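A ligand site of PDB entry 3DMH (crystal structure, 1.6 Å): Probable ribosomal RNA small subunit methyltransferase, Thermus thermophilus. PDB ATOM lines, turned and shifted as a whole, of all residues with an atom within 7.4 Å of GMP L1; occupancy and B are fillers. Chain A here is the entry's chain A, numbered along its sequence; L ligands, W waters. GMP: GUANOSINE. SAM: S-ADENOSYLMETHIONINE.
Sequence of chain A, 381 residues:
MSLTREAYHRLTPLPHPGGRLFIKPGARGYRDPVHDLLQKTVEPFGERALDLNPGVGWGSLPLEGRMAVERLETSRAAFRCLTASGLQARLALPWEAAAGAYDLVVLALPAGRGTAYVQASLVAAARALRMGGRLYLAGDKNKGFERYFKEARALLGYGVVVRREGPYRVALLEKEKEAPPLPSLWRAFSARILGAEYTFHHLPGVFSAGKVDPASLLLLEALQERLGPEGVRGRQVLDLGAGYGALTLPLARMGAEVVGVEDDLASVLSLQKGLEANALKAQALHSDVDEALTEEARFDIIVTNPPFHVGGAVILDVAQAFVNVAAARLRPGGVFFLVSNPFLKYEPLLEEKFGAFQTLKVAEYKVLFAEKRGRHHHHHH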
ATOM      1  N   PHE A 207      18.163   0.639 -17.243  1.00  0.00           N
ATOM      2  CA  PHE A 207      17.036   0.501 -18.171  1.00  0.00           C
ATOM      3  C   PHE A 207      17.254   1.399 -19.387  1.00  0.00           C
ATOM      4  O   PHE A 207      17.623   2.579 -19.248  1.00  0.00           O
ATOM      5  CB  PHE A 207      15.731   0.902 -17.480  1.00  0.00           C
ATOM      6  CG  PHE A 207      14.553   0.925 -18.404  1.00  0.00           C
ATOM      7  CD1 PHE A 207      13.963  -0.265 -18.806  1.00  0.00           C
ATOM      8  CD2 PHE A 207      14.019   2.136 -18.872  1.00  0.00           C
ATOM      9  CE1 PHE A 207      12.864  -0.269 -19.674  1.00  0.00           C
ATOM     10  CE2 PHE A 207      12.922   2.151 -19.728  1.00  0.00           C
ATOM     11  CZ  PHE A 207      12.342   0.940 -20.123  1.00  0.00           C
ATOM     12  N   LYS A 211      19.577   4.824 -25.598  1.00  0.00           N
ATOM     13  CA  LYS A 211      18.490   5.577 -26.232  1.00  0.00           C
ATOM     14  C   LYS A 211      17.357   5.843 -25.258  1.00  0.00           C
ATOM     15  O   LYS A 211      17.133   5.066 -24.345  1.00  0.00           O
ATOM     16  CB  LYS A 211      17.930   4.864 -27.460  1.00  0.00           C
ATOM     17  CG  LYS A 211      17.243   3.535 -27.160  1.00  0.00           C
ATOM     18  CD  LYS A 211      17.052   2.740 -28.466  1.00  0.00           C
ATOM     19  CE  LYS A 211      16.095   1.577 -28.281  1.00  0.00           C
ATOM     20  NZ  LYS A 211      16.626   0.577 -27.304  1.00  0.00           N
ATOM     21  N   ASP A 213      13.777   5.696 -23.911  1.00  0.00           N
ATOM     22  CA  ASP A 213      12.577   4.857 -24.045  1.00  0.00           C
ATOM     23  C   ASP A 213      11.452   5.671 -24.711  1.00  0.00           C
ATOM     24  O   ASP A 213      11.098   6.741 -24.227  1.00  0.00           O
ATOM     25  CB  ASP A 213      12.138   4.369 -22.640  1.00  0.00           C
ATOM     26  CG  ASP A 213      10.912   3.450 -22.667  1.00  0.00           C
ATOM     27  OD1 ASP A 213      10.280   3.247 -23.728  1.00  0.00           O
ATOM     28  OD2 ASP A 213      10.558   2.916 -21.591  1.00  0.00           O
ATOM     29  N   PRO A 214      10.905   5.175 -25.831  1.00  0.00           N
ATOM     30  CA  PRO A 214       9.754   5.851 -26.449  1.00  0.00           C
ATOM     31  C   PRO A 214       8.607   6.098 -25.452  1.00  0.00           C
ATOM     32  O   PRO A 214       7.897   7.094 -25.582  1.00  0.00           O
ATOM     33  CB  PRO A 214       9.330   4.878 -27.555  1.00  0.00           C
ATOM     34  CG  PRO A 214      10.630   4.150 -27.917  1.00  0.00           C
ATOM     35  CD  PRO A 214      11.325   3.988 -26.595  1.00  0.00           C
ATOM     36  N   ALA A 215       8.448   5.240 -24.445  1.00  0.00           N
ATOM     37  CA  ALA A 215       7.398   5.442 -23.449  1.00  0.00           C
ATOM     38  C   ALA A 215       7.645   6.713 -22.625  1.00  0.00           C
ATOM     39  O   ALA A 215       6.704   7.449 -22.297  1.00  0.00           O
ATOM     40  CB  ALA A 215       7.284   4.216 -22.520  1.00  0.00           C
ATOM     41  N   SER A 216       8.911   6.930 -22.276  1.00  0.00           N
ATOM     42  CA  SER A 216       9.299   8.125 -21.521  1.00  0.00           C
ATOM     43  C   SER A 216       9.047   9.401 -22.346  1.00  0.00           C
ATOM     44  O   SER A 216       8.523  10.396 -21.827  1.00  0.00           O
ATOM     45  CB  SER A 216      10.774   8.022 -21.124  1.00  0.00           C
ATOM     46  OG  SER A 216      11.022   6.842 -20.374  1.00  0.00           O
ATOM     47  N   ASN A 305       7.671   6.030 -15.181  1.00  0.00           N
ATOM     48  CA  ASN A 305       7.671   4.948 -16.158  1.00  0.00           C
ATOM     49  C   ASN A 305       8.075   3.710 -15.332  1.00  0.00           C
ATOM     50  O   ASN A 305       9.273   3.463 -15.162  1.00  0.00           O
ATOM     51  CB  ASN A 305       8.705   5.274 -17.243  1.00  0.00           C
ATOM     52  CG  ASN A 305       8.821   4.205 -18.301  1.00  0.00           C
ATOM     53  OD1 ASN A 305       8.125   3.193 -18.262  1.00  0.00           O
ATOM     54  ND2 ASN A 305       9.711   4.425 -19.280  1.00  0.00           N
ATOM     55  N   PRO A 306       7.096   3.001 -14.752  1.00  0.00           N
ATOM     56  CA  PRO A 306       7.473   1.970 -13.768  1.00  0.00           C
ATOM     57  C   PRO A 306       8.169   0.758 -14.356  1.00  0.00           C
ATOM     58  O   PRO A 306       8.047   0.468 -15.566  1.00  0.00           O
ATOM     59  CB  PRO A 306       6.135   1.525 -13.158  1.00  0.00           C
ATOM     60  CG  PRO A 306       5.103   2.429 -13.659  1.00  0.00           C
ATOM     61  CD  PRO A 306       5.629   3.129 -14.894  1.00  0.00           C
ATOM     62  N   PRO A 307       8.841  -0.026 -13.493  1.00  0.00           N
ATOM     63  CA  PRO A 307       9.396  -1.299 -13.944  1.00  0.00           C
ATOM     64  C   PRO A 307       8.278  -2.269 -14.355  1.00  0.00           C
ATOM     65  O   PRO A 307       7.144  -2.126 -13.895  1.00  0.00           O
ATOM     66  CB  PRO A 307      10.130  -1.832 -12.713  1.00  0.00           C
ATOM     67  CG  PRO A 307       9.472  -1.136 -11.560  1.00  0.00           C
ATOM     68  CD  PRO A 307       9.016   0.196 -12.047  1.00  0.00           C
ATOM     69  N   PHE A 308       8.623  -3.241 -15.190  1.00  0.00           N
ATOM     70  CA  PHE A 308       7.622  -4.168 -15.679  1.00  0.00           C
ATOM     71  C   PHE A 308       8.269  -5.515 -15.917  1.00  0.00           C
ATOM     72  O   PHE A 308       9.478  -5.607 -16.122  1.00  0.00           O
ATOM     73  CB  PHE A 308       6.956  -3.629 -16.947  1.00  0.00           C
ATOM     74  CG  PHE A 308       7.923  -3.294 -18.044  1.00  0.00           C
ATOM     75  CD1 PHE A 308       8.212  -4.217 -19.049  1.00  0.00           C
ATOM     76  CD2 PHE A 308       8.545  -2.044 -18.082  1.00  0.00           C
ATOM     77  CE1 PHE A 308       9.108  -3.903 -20.060  1.00  0.00           C
ATOM     78  CE2 PHE A 308       9.449  -1.734 -19.088  1.00  0.00           C
ATOM     79  CZ  PHE A 308       9.735  -2.656 -20.069  1.00  0.00           C
ATOM     80  N   HIS A 309       7.467  -6.567 -15.890  1.00  0.00           N
ATOM     81  CA  HIS A 309       7.968  -7.898 -16.155  1.00  0.00           C
ATOM     82  C   HIS A 309       7.964  -8.101 -17.659  1.00  0.00           C
ATOM     83  O   HIS A 309       6.923  -7.953 -18.303  1.00  0.00           O
ATOM     84  CB  HIS A 309       7.143  -8.956 -15.430  1.00  0.00           C
ATOM     85  CG  HIS A 309       7.593 -10.362 -15.678  1.00  0.00           C
ATOM     86  ND1 HIS A 309       6.732 -11.427 -15.748  1.00  0.00           N
ATOM     87  CD2 HIS A 309       8.842 -10.866 -15.891  1.00  0.00           C
ATOM     88  CE1 HIS A 309       7.408 -12.537 -15.980  1.00  0.00           C
ATOM     89  NE2 HIS A 309       8.691 -12.222 -16.077  1.00  0.00           N
ATOM     90  N   VAL A 310       9.149  -8.404 -18.200  1.00  0.00           N
ATOM     91  CA  VAL A 310       9.396  -8.515 -19.651  1.00  0.00           C
ATOM     92  C   VAL A 310       8.149  -8.790 -20.494  1.00  0.00           C
ATOM     93  O   VAL A 310       7.621  -7.880 -21.142  1.00  0.00           O
ATOM     94  N   GLY A 311       7.686 -10.036 -20.453  1.00  0.00           N
ATOM     95  CA  GLY A 311       6.470 -10.426 -21.160  1.00  0.00           C
ATOM     96  C   GLY A 311       5.307 -10.712 -20.221  1.00  0.00           C
ATOM     97  O   GLY A 311       4.377 -11.443 -20.569  1.00  0.00           O
ATOM     98  N   GLY A 312       5.375 -10.127 -19.033  1.00  0.00           N
ATOM     99  CA  GLY A 312       4.390 -10.357 -17.983  1.00  0.00           C
ATOM    100  C   GLY A 312       3.059  -9.713 -18.252  1.00  0.00           C
ATOM    101  O   GLY A 312       2.950  -8.753 -19.026  1.00  0.00           O
ATOM    102  N   VAL A 339       3.239   5.953 -17.346  1.00  0.00           N
ATOM    103  CA  VAL A 339       3.223   5.381 -18.696  1.00  0.00           C
ATOM    104  C   VAL A 339       3.509   3.885 -18.624  1.00  0.00           C
ATOM    105  O   VAL A 339       4.372   3.454 -17.863  1.00  0.00           O
ATOM    106  CB  VAL A 339       4.193   6.134 -19.650  1.00  0.00           C
ATOM    107  CG1 VAL A 339       5.652   6.013 -19.205  1.00  0.00           C
ATOM    108  CG2 VAL A 339       4.029   5.665 -21.110  1.00  0.00           C
ATOM    109  N   SER A 340       2.761   3.102 -19.424  1.00  0.00           N
ATOM    110  CA  SER A 340       2.972   1.662 -19.430  1.00  0.00           C
ATOM    111  C   SER A 340       2.540   1.005 -20.743  1.00  0.00           C
ATOM    112  O   SER A 340       1.980   1.651 -21.623  1.00  0.00           O
ATOM    113  CB  SER A 340       2.213   1.007 -18.284  1.00  0.00           C
ATOM    114  OG  SER A 340       0.845   0.857 -18.571  1.00  0.00           O
ATOM    115  N   ASN A 341       2.810  -0.281 -20.850  1.00  0.00           N
ATOM    116  CA  ASN A 341       2.260  -1.094 -21.920  1.00  0.00           C
ATOM    117  C   ASN A 341       0.726  -0.952 -21.898  1.00  0.00           C
ATOM    118  O   ASN A 341       0.137  -0.902 -20.822  1.00  0.00           O
ATOM    119  CB  ASN A 341       2.663  -2.558 -21.723  1.00  0.00           C
ATOM    120  CG  ASN A 341       2.058  -3.474 -22.755  1.00  0.00           C
ATOM    121  OD1 ASN A 341       0.909  -3.929 -22.615  1.00  0.00           O
ATOM    122  ND2 ASN A 341       2.813  -3.755 -23.826  1.00  0.00           N
ATOM    123  N   PRO A 342       0.078  -0.882 -23.071  1.00  0.00           N
ATOM    124  CA  PRO A 342      -1.371  -0.661 -23.111  1.00  0.00           C
ATOM    125  C   PRO A 342      -2.250  -1.661 -22.342  1.00  0.00           C
ATOM    126  O   PRO A 342      -3.379  -1.317 -21.984  1.00  0.00           O
ATOM    127  CB  PRO A 342      -1.690  -0.716 -24.624  1.00  0.00           C
ATOM    128  CG  PRO A 342      -0.412  -0.256 -25.251  1.00  0.00           C
ATOM    129  CD  PRO A 342       0.647  -0.949 -24.437  1.00  0.00           C
ATOM    130  N   LEU A 344      -1.458  -3.427 -19.402  1.00  0.00           N
ATOM    131  CA  LEU A 344      -1.263  -3.567 -17.955  1.00  0.00           C
ATOM    132  C   LEU A 344      -2.393  -2.860 -17.204  1.00  0.00           C
ATOM    133  O   LEU A 344      -2.759  -1.729 -17.535  1.00  0.00           O
ATOM    134  CB  LEU A 344       0.126  -3.094 -17.510  1.00  0.00           C
ATOM    135  CG  LEU A 344       1.312  -3.947 -17.975  1.00  0.00           C
ATOM    136  CD1 LEU A 344       2.621  -3.244 -17.640  1.00  0.00           C
ATOM    137  CD2 LEU A 344       1.259  -5.348 -17.361  1.00  0.00           C
ATOM    138  N   TYR A 346      -3.447  -0.898 -14.901  1.00  0.00           N
ATOM    139  CA  TYR A 346      -3.240   0.225 -13.961  1.00  0.00           C
ATOM    140  C   TYR A 346      -4.520   0.984 -13.643  1.00  0.00           C
ATOM    141  O   TYR A 346      -4.643   1.585 -12.588  1.00  0.00           O
ATOM    142  CB  TYR A 346      -2.199   1.197 -14.507  1.00  0.00           C
ATOM    143  CG  TYR A 346      -0.791   0.723 -14.334  1.00  0.00           C
ATOM    144  CD1 TYR A 346      -0.148   0.815 -13.107  1.00  0.00           C
ATOM    145  CD2 TYR A 346      -0.093   0.164 -15.400  1.00  0.00           C
ATOM    146  CE1 TYR A 346       1.156   0.364 -12.956  1.00  0.00           C
ATOM    147  CE2 TYR A 346       1.213  -0.293 -15.257  1.00  0.00           C
ATOM    148  CZ  TYR A 346       1.831  -0.182 -14.038  1.00  0.00           C
ATOM    149  OH  TYR A 346       3.130  -0.630 -13.917  1.00  0.00           O
ATOM    150  N   GLU A 364       1.456   2.850 -28.818  1.00  0.00           N
ATOM    151  CA  GLU A 364       2.432   1.823 -28.483  1.00  0.00           C
ATOM    152  C   GLU A 364       2.470   1.661 -26.960  1.00  0.00           C
ATOM    153  O   GLU A 364       2.688   0.571 -26.443  1.00  0.00           O
ATOM    154  CB  GLU A 364       3.832   2.139 -29.014  1.00  0.00           C
ATOM    155  CG  GLU A 364       4.766   0.905 -28.986  1.00  0.00           C
ATOM    156  CD  GLU A 364       6.156   1.137 -29.585  1.00  0.00           C
ATOM    157  OE1 GLU A 364       6.689   2.275 -29.522  1.00  0.00           O
ATOM    158  OE2 GLU A 364       6.731   0.141 -30.102  1.00  0.00           O
ATOM    159  N   TYR A 365       2.240   2.782 -26.273  1.00  0.00           N
ATOM    160  CA  TYR A 365       2.114   2.807 -24.811  1.00  0.00           C
ATOM    161  C   TYR A 365       0.901   3.625 -24.430  1.00  0.00           C
ATOM    162  O   TYR A 365       0.320   4.341 -25.266  1.00  0.00           O
ATOM    163  CB  TYR A 365       3.354   3.411 -24.147  1.00  0.00           C
ATOM    164  CG  TYR A 365       4.627   2.781 -24.644  1.00  0.00           C
ATOM    165  CD1 TYR A 365       5.159   1.657 -24.012  1.00  0.00           C
ATOM    166  CD2 TYR A 365       5.275   3.290 -25.760  1.00  0.00           C
ATOM    167  CE1 TYR A 365       6.317   1.056 -24.512  1.00  0.00           C
ATOM    168  CE2 TYR A 365       6.418   2.710 -26.243  1.00  0.00           C
ATOM    169  CZ  TYR A 365       6.935   1.606 -25.630  1.00  0.00           C
ATOM    170  OH  TYR A 365       8.087   1.057 -26.120  1.00  0.00           O
HETATM  171  C4' GMP L   1       8.576  -2.465 -26.393  1.00  0.00           C
HETATM  172  O4' GMP L   1       8.007  -1.947 -25.181  1.00  0.00           O
HETATM  173  C3' GMP L   1       9.585  -3.526 -25.958  1.00  0.00           C
HETATM  174  O3' GMP L   1      10.879  -2.913 -25.959  1.00  0.00           O
HETATM  175  C2' GMP L   1       9.178  -3.864 -24.542  1.00  0.00           C
HETATM  176  O2' GMP L   1      10.299  -4.288 -23.765  1.00  0.00           O
HETATM  177  C1' GMP L   1       8.635  -2.543 -24.035  1.00  0.00           C
HETATM  178  N9  GMP L   1       7.615  -2.619 -22.971  1.00  0.00           N
HETATM  179  C8  GMP L   1       6.700  -3.587 -22.755  1.00  0.00           C
HETATM  180  N7  GMP L   1       5.921  -3.300 -21.684  1.00  0.00           N
HETATM  181  C5  GMP L   1       6.318  -2.097 -21.204  1.00  0.00           C
HETATM  182  C6  GMP L   1       5.933  -1.193 -20.095  1.00  0.00           C
HETATM  183  O6  GMP L   1       5.001  -1.483 -19.321  1.00  0.00           O
HETATM  184  N1  GMP L   1       6.629  -0.045 -19.955  1.00  0.00           N
HETATM  185  C2  GMP L   1       7.649   0.301 -20.775  1.00  0.00           C
HETATM  186  N2  GMP L   1       8.329   1.461 -20.583  1.00  0.00           N
HETATM  187  N3  GMP L   1       8.056  -0.481 -21.803  1.00  0.00           N
HETATM  188  C4  GMP L   1       7.439  -1.661 -22.064  1.00  0.00           C
HETATM  189  N   SAM L   2      12.539   6.854 -15.478  1.00  0.00           N
HETATM  190  CA  SAM L   2      13.538   6.136 -16.336  1.00  0.00           C
HETATM  191  C   SAM L   2      13.144   6.293 -17.788  1.00  0.00           C
HETATM  192  O   SAM L   2      11.998   6.720 -17.992  1.00  0.00           O
HETATM  193  OXT SAM L   2      13.929   5.948 -18.684  1.00  0.00           O
HETATM  194  CB  SAM L   2      13.602   4.647 -15.995  1.00  0.00           C
HETATM  195  CG  SAM L   2      12.290   3.871 -16.171  1.00  0.00           C
HETATM  196  SD  SAM L   2      12.522   2.091 -15.855  1.00  0.00           S
HETATM  197  CE  SAM L   2      11.106   1.381 -16.747  1.00  0.00           C
HETATM  198  C5' SAM L   2      11.984   1.822 -14.142  1.00  0.00           C
HETATM  199  C4' SAM L   2      13.038   2.257 -13.128  1.00  0.00           C
HETATM  200  O4' SAM L   2      12.517   1.885 -11.861  1.00  0.00           O
HETATM  201  C3' SAM L   2      14.411   1.592 -13.297  1.00  0.00           C
HETATM  202  O3' SAM L   2      15.452   2.554 -13.394  1.00  0.00           O
HETATM  203  C2' SAM L   2      14.525   0.719 -12.045  1.00  0.00           C
HETATM  204  O2' SAM L   2      15.849   0.501 -11.576  1.00  0.00           O
HETATM  205  C1' SAM L   2      13.640   1.526 -11.094  1.00  0.00           C
HETATM  206  N9  SAM L   2      13.248   0.754  -9.935  1.00  0.00           N
HETATM  207  C8  SAM L   2      13.023  -0.616  -9.834  1.00  0.00           C
HETATM  208  N7  SAM L   2      12.638  -0.907  -8.565  1.00  0.00           N
HETATM  209  C5  SAM L   2      12.640   0.271  -7.842  1.00  0.00           C
HETATM  210  C6  SAM L   2      12.386   0.585  -6.512  1.00  0.00           C
HETATM  211  N6  SAM L   2      12.069  -0.361  -5.612  1.00  0.00           N
HETATM  212  N1  SAM L   2      12.477   1.906  -6.134  1.00  0.00           N
HETATM  213  C2  SAM L   2      12.836   2.890  -7.026  1.00  0.00           C
HETATM  214  N3  SAM L   2      13.149   2.601  -8.346  1.00  0.00           N
HETATM  215  C4  SAM L   2      13.030   1.304  -8.724  1.00  0.00           C
HETATM  216  O   HOH W   1       4.380  -5.390 -20.468  1.00  0.00           O
HETATM  217  O   HOH W   2       4.487  -0.798 -16.588  1.00  0.00           O
HETATM  218  O   HOH W   3      12.268  -0.509 -23.871  1.00  0.00           O
HETATM  219  O   HOH W   4       9.704   0.561 -23.914  1.00  0.00           O
HETATM  220  O   HOH W   5       6.198   1.127 -17.524  1.00  0.00           O
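Residues that only touch GMP L1: Ala 215 (3.5 Å), Phe 308 (3.2 Å), Ser 340 (3.7 Å) and Leu 344 (3.4 Å).
Hydrophobic or aromatic side chains that line GMP L1: Ala 215, Phe 308, Leu 344 and Tyr 365.
Within 4 Å of GMP L1: Asp 213, Ala 215, Asn 305, Phe 308, Ser 340, Asn 341, Leu 344 and Tyr 365.
Water W2 bridges an oxygen (O6) of GMP L1 and the side-chain hydroxyl (OH) of Tyr 346.
Water W4 lies within hydrogen-bond range of OD1 of Asp 213, OH of Tyr 365 and N3 of GMP L1.
The side-chain carboxylate (OD2) of Asp 213 is in hydrogen-bond range of the side-chain amide nitrogen (ND2) of Asn 305 (2.9 Å).
OD1 of Asp 213 lies within hydrogen-bond range of N of Ala 215.
The side-chain hydroxyl (OG) of Ser 216 lies within hydrogen-bond range of the side-chain amide nitrogen (ND2) of Asn 305 (3.0 Å).
OD1 of Asn 305 sits at hydrogen-bond distance from N2 of GMP L1 (2.9 Å).
O of SAM L2 lies within hydrogen-bond range of OG of Ser 216, 2.6 Å away.
ND2 of Asn 305 sits at hydrogen-bond distance from O of SAM L2 (3.5 Å).
The backbone NH of Asn 341 sits at hydrogen-bond distance from an oxygen (O6) of GMP L1 (2.9 Å).
The side-chain hydroxyl of Tyr 365 lies within hydrogen-bond range of an oxygen (O4') of GMP L1, 3.1 Å away.
A nitrogen (N2) of GMP L1 sits at hydrogen-bond distance from the side-chain carboxylate (OD2) of Asp 213 (2.8 Å).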
